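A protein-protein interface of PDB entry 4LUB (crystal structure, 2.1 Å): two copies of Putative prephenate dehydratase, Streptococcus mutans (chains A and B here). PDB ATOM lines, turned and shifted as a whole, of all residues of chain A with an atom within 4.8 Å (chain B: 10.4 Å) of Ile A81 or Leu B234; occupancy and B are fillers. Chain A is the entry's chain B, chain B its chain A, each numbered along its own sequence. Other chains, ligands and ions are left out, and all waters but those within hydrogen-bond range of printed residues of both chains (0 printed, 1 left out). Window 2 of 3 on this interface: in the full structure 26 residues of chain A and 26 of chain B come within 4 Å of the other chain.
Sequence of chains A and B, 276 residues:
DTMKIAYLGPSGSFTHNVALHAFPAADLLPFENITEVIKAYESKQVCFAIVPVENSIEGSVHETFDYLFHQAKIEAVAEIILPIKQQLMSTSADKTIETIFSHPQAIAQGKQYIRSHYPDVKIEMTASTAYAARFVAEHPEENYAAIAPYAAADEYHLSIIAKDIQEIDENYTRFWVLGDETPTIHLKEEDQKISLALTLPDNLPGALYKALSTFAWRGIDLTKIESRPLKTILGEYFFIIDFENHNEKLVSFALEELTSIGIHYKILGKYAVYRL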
ATOM      1  N   GLU A  54      17.058  28.727  20.792  1.00  0.00           N
ATOM      2  CA  GLU A  54      17.515  28.510  19.426  1.00  0.00           C
ATOM      3  C   GLU A  54      17.228  29.675  18.501  1.00  0.00           C
ATOM      4  O   GLU A  54      16.135  30.224  18.530  1.00  0.00           O
ATOM      5  CB  GLU A  54      16.871  27.247  18.834  1.00  0.00           C
ATOM      6  CG  GLU A  54      17.326  26.956  17.407  1.00  0.00           C
ATOM      7  CD  GLU A  54      16.790  25.652  16.869  1.00  0.00           C
ATOM      8  OE1 GLU A  54      16.151  24.913  17.646  1.00  0.00           O
ATOM      9  OE2 GLU A  54      17.025  25.360  15.676  1.00  0.00           O
ATOM     10  N   ASN A  55      18.190  30.001  17.642  1.00  0.00           N
ATOM     11  CA  ASN A  55      18.028  31.066  16.658  1.00  0.00           C
ATOM     12  C   ASN A  55      18.098  30.494  15.250  1.00  0.00           C
ATOM     13  O   ASN A  55      18.844  29.548  14.989  1.00  0.00           O
ATOM     14  CB  ASN A  55      19.090  32.152  16.842  1.00  0.00           C
ATOM     15  CG  ASN A  55      18.962  33.267  15.822  1.00  0.00           C
ATOM     16  OD1 ASN A  55      19.574  33.210  14.757  1.00  0.00           O
ATOM     17  ND2 ASN A  55      18.132  34.264  16.119  1.00  0.00           N
ATOM     18  N   SER A  56      17.329  31.083  14.343  1.00  0.00           N
ATOM     19  CA  SER A  56      17.218  30.599  12.970  1.00  0.00           C
ATOM     20  C   SER A  56      18.531  30.690  12.180  1.00  0.00           C
ATOM     21  O   SER A  56      18.678  30.039  11.142  1.00  0.00           O
ATOM     22  CB  SER A  56      16.088  31.344  12.246  1.00  0.00           C
ATOM     23  OG  SER A  56      16.446  32.672  11.936  1.00  0.00           O
ATOM     24  N   GLU A  79       6.793  27.258  24.764  1.00  0.00           N
ATOM     25  CA  GLU A  79       7.727  27.887  23.836  1.00  0.00           C
ATOM     26  C   GLU A  79       7.115  29.107  23.143  1.00  0.00           C
ATOM     27  O   GLU A  79       5.999  29.035  22.641  1.00  0.00           O
ATOM     28  CB  GLU A  79       8.181  26.878  22.782  1.00  0.00           C
ATOM     29  CG  GLU A  79       9.235  27.407  21.824  1.00  0.00           C
ATOM     30  CD  GLU A  79       9.632  26.366  20.800  1.00  0.00           C
ATOM     31  OE1 GLU A  79      10.135  25.308  21.218  1.00  0.00           O
ATOM     32  OE2 GLU A  79       9.518  26.626  19.587  1.00  0.00           O
ATOM     33  N   ILE A  80       7.846  30.219  23.123  1.00  0.00           N
ATOM     34  CA  ILE A  80       7.424  31.408  22.376  1.00  0.00           C
ATOM     35  C   ILE A  80       8.466  31.749  21.321  1.00  0.00           C
ATOM     36  O   ILE A  80       9.649  31.886  21.625  1.00  0.00           O
ATOM     37  CB  ILE A  80       7.178  32.629  23.295  1.00  0.00           C
ATOM     38  CG1 ILE A  80       6.012  32.342  24.242  1.00  0.00           C
ATOM     39  CG2 ILE A  80       6.843  33.870  22.466  1.00  0.00           C
ATOM     40  CD1 ILE A  80       6.019  33.176  25.512  1.00  0.00           C
ATOM     41  N   ILE A  81       8.025  31.845  20.074  1.00  0.00           N
ATOM     42  CA  ILE A  81       8.893  32.266  18.980  1.00  0.00           C
ATOM     43  C   ILE A  81       8.795  33.760  18.679  1.00  0.00           C
ATOM     44  O   ILE A  81       7.712  34.288  18.443  1.00  0.00           O
ATOM     45  CB  ILE A  81       8.588  31.467  17.705  1.00  0.00           C
ATOM     46  CG1 ILE A  81       8.812  29.977  17.969  1.00  0.00           C
ATOM     47  CG2 ILE A  81       9.506  31.905  16.570  1.00  0.00           C
ATOM     48  CD1 ILE A  81       8.498  29.087  16.775  1.00  0.00           C
ATOM     49  N   LEU A  82       9.944  34.426  18.713  1.00  0.00           N
ATOM     50  CA  LEU A  82      10.063  35.864  18.459  1.00  0.00           C
ATOM     51  C   LEU A  82      10.749  36.203  17.147  1.00  0.00           C
ATOM     52  O   LEU A  82      11.835  35.704  16.872  1.00  0.00           O
ATOM     53  CB  LEU A  82      10.845  36.539  19.593  1.00  0.00           C
ATOM     54  CG  LEU A  82      10.773  38.070  19.695  1.00  0.00           C
ATOM     55  CD1 LEU A  82       9.436  38.574  20.221  1.00  0.00           C
ATOM     56  CD2 LEU A  82      11.928  38.602  20.539  1.00  0.00           C
ATOM     57  N   PRO A  83      10.118  37.071  16.341  1.00  0.00           N
ATOM     58  CA  PRO A  83      10.814  37.704  15.217  1.00  0.00           C
ATOM     59  C   PRO A  83      11.903  38.655  15.704  1.00  0.00           C
ATOM     60  O   PRO A  83      11.684  39.404  16.659  1.00  0.00           O
ATOM     61  CB  PRO A  83       9.706  38.475  14.489  1.00  0.00           C
ATOM     62  CG  PRO A  83       8.571  38.556  15.464  1.00  0.00           C
ATOM     63  CD  PRO A  83       8.670  37.343  16.324  1.00  0.00           C
ATOM     64  N   TYR A 172      14.506  34.740  13.518  1.00  0.00           N
ATOM     65  CA  TYR A 172      13.614  34.103  14.490  1.00  0.00           C
ATOM     66  C   TYR A 172      14.317  33.305  15.582  1.00  0.00           C
ATOM     67  O   TYR A 172      15.238  32.530  15.323  1.00  0.00           O
ATOM     68  CB  TYR A 172      12.607  33.190  13.797  1.00  0.00           C
ATOM     69  CG  TYR A 172      11.507  33.927  13.073  1.00  0.00           C
ATOM     70  CD1 TYR A 172      10.333  34.270  13.732  1.00  0.00           C
ATOM     71  CD2 TYR A 172      11.637  34.286  11.739  1.00  0.00           C
ATOM     72  CE1 TYR A 172       9.319  34.946  13.084  1.00  0.00           C
ATOM     73  CE2 TYR A 172      10.627  34.963  11.078  1.00  0.00           C
ATOM     74  CZ  TYR A 172       9.468  35.289  11.757  1.00  0.00           C
ATOM     75  OH  TYR A 172       8.454  35.963  11.110  1.00  0.00           O
ATOM     76  N   THR A 173      13.850  33.492  16.812  1.00  0.00           N
ATOM     77  CA  THR A 173      14.420  32.812  17.964  1.00  0.00           C
ATOM     78  C   THR A 173      13.328  32.093  18.742  1.00  0.00           C
ATOM     79  O   THR A 173      12.229  32.624  18.941  1.00  0.00           O
ATOM     80  CB  THR A 173      15.152  33.790  18.903  1.00  0.00           C
ATOM     81  OG1 THR A 173      16.194  34.451  18.179  1.00  0.00           O
ATOM     82  CG2 THR A 173      15.767  33.059  20.107  1.00  0.00           C
ATOM     83  N   ARG A 174      13.665  30.904  19.225  1.00  0.00           N
ATOM     84  CA  ARG A 174      12.778  30.133  20.073  1.00  0.00           C
ATOM     85  C   ARG A 174      13.174  30.431  21.513  1.00  0.00           C
ATOM     86  O   ARG A 174      14.353  30.389  21.849  1.00  0.00           O
ATOM     87  CB  ARG A 174      12.921  28.632  19.773  1.00  0.00           C
ATOM     88  CG  ARG A 174      12.548  28.254  18.351  1.00  0.00           C
ATOM     89  CD  ARG A 174      12.940  26.820  17.997  1.00  0.00           C
ATOM     90  NE  ARG A 174      12.103  25.848  18.696  1.00  0.00           N
ATOM     91  CZ  ARG A 174      12.496  24.628  19.044  1.00  0.00           C
ATOM     92  NH1 ARG A 174      13.707  24.202  18.714  1.00  0.00           N
ATOM     93  NH2 ARG A 174      11.660  23.817  19.679  1.00  0.00           N
ATOM     94  N   GLU A 190       0.793  27.325  17.558  1.00  0.00           N
ATOM     95  CA  GLU A 190       1.253  26.942  16.239  1.00  0.00           C
ATOM     96  C   GLU A 190       1.679  25.465  16.188  1.00  0.00           C
ATOM     97  O   GLU A 190       1.720  24.862  15.113  1.00  0.00           O
ATOM     98  CB  GLU A 190       2.378  27.894  15.824  1.00  0.00           C
ATOM     99  CG  GLU A 190       3.550  27.306  15.090  1.00  0.00           C
ATOM    100  CD  GLU A 190       4.577  28.366  14.745  1.00  0.00           C
ATOM    101  OE1 GLU A 190       4.198  29.559  14.690  1.00  0.00           O
ATOM    102  OE2 GLU A 190       5.755  28.007  14.534  1.00  0.00           O
ATOM    103  N   VAL A 273       3.774  25.464  21.333  1.00  0.00           N
ATOM    104  CA  VAL A 273       4.536  26.502  20.655  1.00  0.00           C
ATOM    105  C   VAL A 273       3.649  27.680  20.269  1.00  0.00           C
ATOM    106  O   VAL A 273       2.652  27.509  19.575  1.00  0.00           O
ATOM    107  CB  VAL A 273       5.228  25.956  19.382  1.00  0.00           C
ATOM    108  CG1 VAL A 273       6.074  27.045  18.718  1.00  0.00           C
ATOM    109  CG2 VAL A 273       6.047  24.705  19.714  1.00  0.00           C
ATOM    110  N   TYR A 274       4.037  28.870  20.709  1.00  0.00           N
ATOM    111  CA  TYR A 274       3.333  30.105  20.387  1.00  0.00           C
ATOM    112  C   TYR A 274       4.263  30.974  19.551  1.00  0.00           C
ATOM    113  O   TYR A 274       5.479  30.874  19.692  1.00  0.00           O
ATOM    114  CB  TYR A 274       2.914  30.832  21.659  1.00  0.00           C
ATOM    115  CG  TYR A 274       2.126  29.976  22.628  1.00  0.00           C
ATOM    116  CD1 TYR A 274       0.752  29.821  22.497  1.00  0.00           C
ATOM    117  CD2 TYR A 274       2.764  29.324  23.680  1.00  0.00           C
ATOM    118  CE1 TYR A 274       0.031  29.035  23.390  1.00  0.00           C
ATOM    119  CE2 TYR A 274       2.052  28.544  24.581  1.00  0.00           C
ATOM    120  CZ  TYR A 274       0.689  28.403  24.431  1.00  0.00           C
ATOM    121  OH  TYR A 274      -0.016  27.625  25.323  1.00  0.00           O
ATOM    122  N   ARG A 275       3.721  31.773  18.637  1.00  0.00           N
ATOM    123  CA  ARG A 275       4.589  32.608  17.811  1.00  0.00           C
ATOM    124  C   ARG A 275       4.444  34.084  18.170  1.00  0.00           C
ATOM    125  O   ARG A 275       3.356  34.651  18.064  1.00  0.00           O
ATOM    126  CB  ARG A 275       4.305  32.393  16.322  1.00  0.00           C
ATOM    127  CG  ARG A 275       5.249  33.166  15.401  1.00  0.00           C
ATOM    128  CD  ARG A 275       5.189  32.648  13.969  1.00  0.00           C
ATOM    129  NE  ARG A 275       5.831  31.341  13.824  1.00  0.00           N
ATOM    130  CZ  ARG A 275       7.043  31.143  13.309  1.00  0.00           C
ATOM    131  NH1 ARG A 275       7.763  32.167  12.874  1.00  0.00           N
ATOM    132  NH2 ARG A 275       7.535  29.913  13.222  1.00  0.00           N
ATOM    133  N   ASP B 202      12.376  18.541   1.017  1.00  0.00           N
ATOM    134  CA  ASP B 202      11.615  19.693   1.510  1.00  0.00           C
ATOM    135  C   ASP B 202      12.303  20.329   2.727  1.00  0.00           C
ATOM    136  O   ASP B 202      11.681  21.057   3.495  1.00  0.00           O
ATOM    137  CB  ASP B 202      10.177  19.289   1.838  1.00  0.00           C
ATOM    138  CG  ASP B 202       9.447  18.710   0.646  1.00  0.00           C
ATOM    139  OD1 ASP B 202       9.344  19.404  -0.386  1.00  0.00           O
ATOM    140  OD2 ASP B 202       8.957  17.563   0.750  1.00  0.00           O
ATOM    141  N   ASN B 203      13.595  20.046   2.875  1.00  0.00           N
ATOM    142  CA  ASN B 203      14.410  20.401   4.050  1.00  0.00           C
ATOM    143  C   ASN B 203      13.852  20.177   5.481  1.00  0.00           C
ATOM    144  O   ASN B 203      14.266  20.869   6.413  1.00  0.00           O
ATOM    145  CB  ASN B 203      14.796  21.877   3.918  1.00  0.00           C
ATOM    146  CG  ASN B 203      15.646  22.139   2.690  1.00  0.00           C
ATOM    147  OD1 ASN B 203      16.670  21.481   2.478  1.00  0.00           O
ATOM    148  ND2 ASN B 203      15.227  23.098   1.873  1.00  0.00           N
ATOM    149  N   LEU B 204      12.944  19.224   5.680  1.00  0.00           N
ATOM    150  CA  LEU B 204      12.508  18.908   7.050  1.00  0.00           C
ATOM    151  C   LEU B 204      13.334  17.738   7.601  1.00  0.00           C
ATOM    152  O   LEU B 204      13.579  16.753   6.888  1.00  0.00           O
ATOM    153  CB  LEU B 204      11.012  18.592   7.164  1.00  0.00           C
ATOM    154  CG  LEU B 204       9.950  19.238   6.279  1.00  0.00           C
ATOM    155  CD1 LEU B 204       9.874  18.461   4.980  1.00  0.00           C
ATOM    156  CD2 LEU B 204       8.597  19.193   6.942  1.00  0.00           C
ATOM    157  N   PRO B 205      13.801  17.867   8.851  1.00  0.00           N
ATOM    158  CA  PRO B 205      14.638  16.874   9.537  1.00  0.00           C
ATOM    159  C   PRO B 205      13.974  15.497   9.629  1.00  0.00           C
ATOM    160  O   PRO B 205      14.672  14.512   9.872  1.00  0.00           O
ATOM    161  CB  PRO B 205      14.815  17.459  10.933  1.00  0.00           C
ATOM    162  CG  PRO B 205      14.499  18.892  10.822  1.00  0.00           C
ATOM    163  CD  PRO B 205      13.600  19.090   9.648  1.00  0.00           C
ATOM    164  N   ARG B 228      23.130  22.097  11.452  1.00  0.00           N
ATOM    165  CA  ARG B 228      23.359  23.537  11.381  1.00  0.00           C
ATOM    166  C   ARG B 228      22.148  24.109  10.667  1.00  0.00           C
ATOM    167  O   ARG B 228      21.603  23.460   9.766  1.00  0.00           O
ATOM    168  CB  ARG B 228      24.642  23.874  10.616  1.00  0.00           C
ATOM    169  CG  ARG B 228      25.972  23.590  11.339  1.00  0.00           C
ATOM    170  CD  ARG B 228      26.083  24.374  12.653  1.00  0.00           C
ATOM    171  NE  ARG B 228      26.072  25.805  12.377  1.00  0.00           N
ATOM    172  CZ  ARG B 228      25.512  26.731  13.146  1.00  0.00           C
ATOM    173  NH1 ARG B 228      24.925  26.395  14.287  1.00  0.00           N
ATOM    174  NH2 ARG B 228      25.563  28.007  12.778  1.00  0.00           N
ATOM    175  N   PRO B 229      21.706  25.310  11.062  1.00  0.00           N
ATOM    176  CA  PRO B 229      20.631  25.973  10.312  1.00  0.00           C
ATOM    177  C   PRO B 229      20.967  26.116   8.827  1.00  0.00           C
ATOM    178  O   PRO B 229      22.115  26.396   8.482  1.00  0.00           O
ATOM    179  CB  PRO B 229      20.515  27.347  10.985  1.00  0.00           C
ATOM    180  CG  PRO B 229      21.225  27.201  12.305  1.00  0.00           C
ATOM    181  CD  PRO B 229      22.291  26.184  12.091  1.00  0.00           C
ATOM    182  N   LEU B 230      19.981  25.883   7.969  1.00  0.00           N
ATOM    183  CA  LEU B 230      20.122  26.148   6.539  1.00  0.00           C
ATOM    184  C   LEU B 230      20.215  27.642   6.219  1.00  0.00           C
ATOM    185  O   LEU B 230      20.523  28.017   5.090  1.00  0.00           O
ATOM    186  CB  LEU B 230      18.947  25.530   5.770  1.00  0.00           C
ATOM    187  CG  LEU B 230      19.133  25.086   4.318  1.00  0.00           C
ATOM    188  CD1 LEU B 230      20.425  24.318   4.121  1.00  0.00           C
ATOM    189  CD2 LEU B 230      17.939  24.243   3.883  1.00  0.00           C
ATOM    190  N   LYS B 231      19.941  28.484   7.213  1.00  0.00           N
ATOM    191  CA  LYS B 231      19.830  29.938   7.038  1.00  0.00           C
ATOM    192  C   LYS B 231      18.759  30.296   6.012  1.00  0.00           C
ATOM    193  O   LYS B 231      18.923  31.222   5.213  1.00  0.00           O
ATOM    194  CB  LYS B 231      21.164  30.568   6.604  1.00  0.00           C
ATOM    195  CG  LYS B 231      22.413  29.964   7.215  1.00  0.00           C
ATOM    196  CD  LYS B 231      22.773  30.642   8.513  1.00  0.00           C
ATOM    197  CE  LYS B 231      24.277  30.663   8.702  1.00  0.00           C
ATOM    198  NZ  LYS B 231      24.656  30.465  10.124  1.00  0.00           N
ATOM    199  N   THR B 232      17.646  29.578   6.065  1.00  0.00           N
ATOM    200  CA  THR B 232      16.488  29.886   5.240  1.00  0.00           C
ATOM    201  C   THR B 232      15.353  30.301   6.160  1.00  0.00           C
ATOM    202  O   THR B 232      15.080  31.489   6.322  1.00  0.00           O
ATOM    203  CB  THR B 232      16.068  28.695   4.383  1.00  0.00           C
ATOM    204  OG1 THR B 232      15.980  27.525   5.210  1.00  0.00           O
ATOM    205  CG2 THR B 232      17.088  28.460   3.274  1.00  0.00           C
ATOM    206  N   ILE B 233      14.694  29.321   6.769  1.00  0.00           N
ATOM    207  CA  ILE B 233      13.770  29.598   7.859  1.00  0.00           C
ATOM    208  C   ILE B 233      14.064  28.714   9.061  1.00  0.00           C
ATOM    209  O   ILE B 233      14.745  27.697   8.947  1.00  0.00           O
ATOM    210  CB  ILE B 233      12.306  29.403   7.421  1.00  0.00           C
ATOM    211  CG1 ILE B 233      12.087  27.978   6.910  1.00  0.00           C
ATOM    212  CG2 ILE B 233      11.924  30.417   6.350  1.00  0.00           C
ATOM    213  CD1 ILE B 233      10.714  27.418   7.203  1.00  0.00           C
ATOM    214  N   LEU B 234      13.565  29.131  10.218  1.00  0.00           N
ATOM    215  CA  LEU B 234      13.550  28.301  11.413  1.00  0.00           C
ATOM    216  C   LEU B 234      12.954  26.915  11.175  1.00  0.00           C
ATOM    217  O   LEU B 234      11.832  26.793  10.699  1.00  0.00           O
ATOM    218  CB  LEU B 234      12.778  29.014  12.523  1.00  0.00           C
ATOM    219  CG  LEU B 234      12.935  28.506  13.954  1.00  0.00           C
ATOM    220  CD1 LEU B 234      14.385  28.542  14.413  1.00  0.00           C
ATOM    221  CD2 LEU B 234      12.065  29.349  14.874  1.00  0.00           C
ATOM    222  N   GLY B 235      13.707  25.876  11.533  1.00  0.00           N
ATOM    223  CA  GLY B 235      13.253  24.509  11.356  1.00  0.00           C
ATOM    224  C   GLY B 235      13.792  23.830  10.113  1.00  0.00           C
ATOM    225  O   GLY B 235      13.501  22.660   9.871  1.00  0.00           O
ATOM    226  N   GLU B 236      14.604  24.556   9.357  1.00  0.00           N
ATOM    227  CA  GLU B 236      15.319  24.000   8.219  1.00  0.00           C
ATOM    228  C   GLU B 236      16.815  23.943   8.509  1.00  0.00           C
ATOM    229  O   GLU B 236      17.407  24.927   8.944  1.00  0.00           O
ATOM    230  CB  GLU B 236      15.062  24.821   6.958  1.00  0.00           C
ATOM    231  CG  GLU B 236      13.635  24.749   6.455  1.00  0.00           C
ATOM    232  CD  GLU B 236      13.489  25.248   5.032  1.00  0.00           C
ATOM    233  OE1 GLU B 236      14.469  25.777   4.479  1.00  0.00           O
ATOM    234  OE2 GLU B 236      12.389  25.107   4.470  1.00  0.00           O
ATOM    235  N   TYR B 237      17.409  22.782   8.258  1.00  0.00           N
ATOM    236  CA  TYR B 237      18.809  22.532   8.562  1.00  0.00           C
ATOM    237  C   TYR B 237      19.516  21.757   7.463  1.00  0.00           C
ATOM    238  O   TYR B 237      18.887  21.181   6.589  1.00  0.00           O
ATOM    239  CB  TYR B 237      18.931  21.717   9.852  1.00  0.00           C
ATOM    240  CG  TYR B 237      18.107  22.215  11.013  1.00  0.00           C
ATOM    241  CD1 TYR B 237      18.654  23.064  11.958  1.00  0.00           C
ATOM    242  CD2 TYR B 237      16.786  21.833  11.164  1.00  0.00           C
ATOM    243  CE1 TYR B 237      17.909  23.517  13.023  1.00  0.00           C
ATOM    244  CE2 TYR B 237      16.032  22.283  12.224  1.00  0.00           C
ATOM    245  CZ  TYR B 237      16.599  23.128  13.148  1.00  0.00           C
ATOM    246  OH  TYR B 237      15.851  23.573  14.201  1.00  0.00           O
ATOM    247  N   PHE B 238      20.840  21.739   7.538  1.00  0.00           N
ATOM    248  CA  PHE B 238      21.643  20.745   6.849  1.00  0.00           C
ATOM    249  C   PHE B 238      22.323  19.877   7.906  1.00  0.00           C
ATOM    250  O   PHE B 238      22.564  20.330   9.016  1.00  0.00           O
ATOM    251  CB  PHE B 238      22.630  21.365   5.852  1.00  0.00           C
ATOM    252  CG  PHE B 238      23.809  22.055   6.479  1.00  0.00           C
ATOM    253  CD1 PHE B 238      24.964  21.354   6.783  1.00  0.00           C
ATOM    254  CD2 PHE B 238      23.780  23.417   6.717  1.00  0.00           C
ATOM    255  CE1 PHE B 238      26.056  21.998   7.339  1.00  0.00           C
ATOM    256  CE2 PHE B 238      24.867  24.065   7.270  1.00  0.00           C
ATOM    257  CZ  PHE B 238      26.006  23.356   7.582  1.00  0.00           C
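Of the 15 printed residues of chain B, 3 touch a printed residue of chain A. Hydrophobic or aromatic side chains of chain B within 4 Å of the printed part of chain A: Pro B229, Leu B234 and Tyr B237. Printed residues of chain A that touch a printed residue of chain B: Glu A54, Ser A56, Ile A81 and Arg A174. Among the printed residues, no Asp or Glu carboxylate lies within 4 Å of a Lys or Arg side-chain nitrogen of the other chain.
Among the printed residues, pairs that only touch across the chains: Ser A56 with Pro B229 (3.3 Å), Ser A56 with Leu B234 (3.8 Å), Ile A81 with Leu B234 (3.99 Å) and Arg A174 with Leu B234 (3.7 Å).
OE1 of Glu A79 is in salt-bridge range of NH2 of Arg A174 (2.6 Å). The backbone NH (N) of Ser A56 sits at hydrogen-bond distance from the backbone carbonyl oxygen (O) of Tyr A172 (2.7 Å). OE1 of Glu A54 lies within salt-bridge range of NH1 of Arg A174 (2.8 Å). The backbone NH (N) of Ile A81 is in hydrogen-bond range of the backbone carbonyl oxygen (O) of Tyr A274 (2.8 Å).
Printed residues of chain B within 4 Å of Ile A81: Leu B234. Of the printed residues of chain A, Leu B234 touches Ser A56, Ile A81 and Arg A174. Ser A56 touches just these residues of chain B: Pro B229 (3.3 Å) and Leu B234 (3.8 Å). No residue of chain B comes within 4 Å of Ile A80. No residue of chain B comes within 4 Å of Leu A82. Printed residues of chain A within 4 Å of Tyr B237: Glu A54. Of the printed residues of chain B, Glu A54 touches Tyr B237 (2.6 Å). Of the printed residues of chain A, Pro B229 touches Ser A56 (3.3 Å). Of the printed residues of chain B, Arg A174 touches Leu B234. The nearest printed residue of chain B that does not touch Ile A81 is Gly B235 (8.1 Å). The nearest printed residue of chain A that does not touch Leu B234 is Tyr A172 (4.03 Å).
No position is printed for both chains. Of the 5 pairs that touch across the chains among the printed residues, none has its exchanged pair printed and touching as well.
The side-chain hydroxyl (OH) of Tyr B237 is in hydrogen-bond range of the side-chain carboxylate (OE2) of Glu A54 (2.6 Å).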
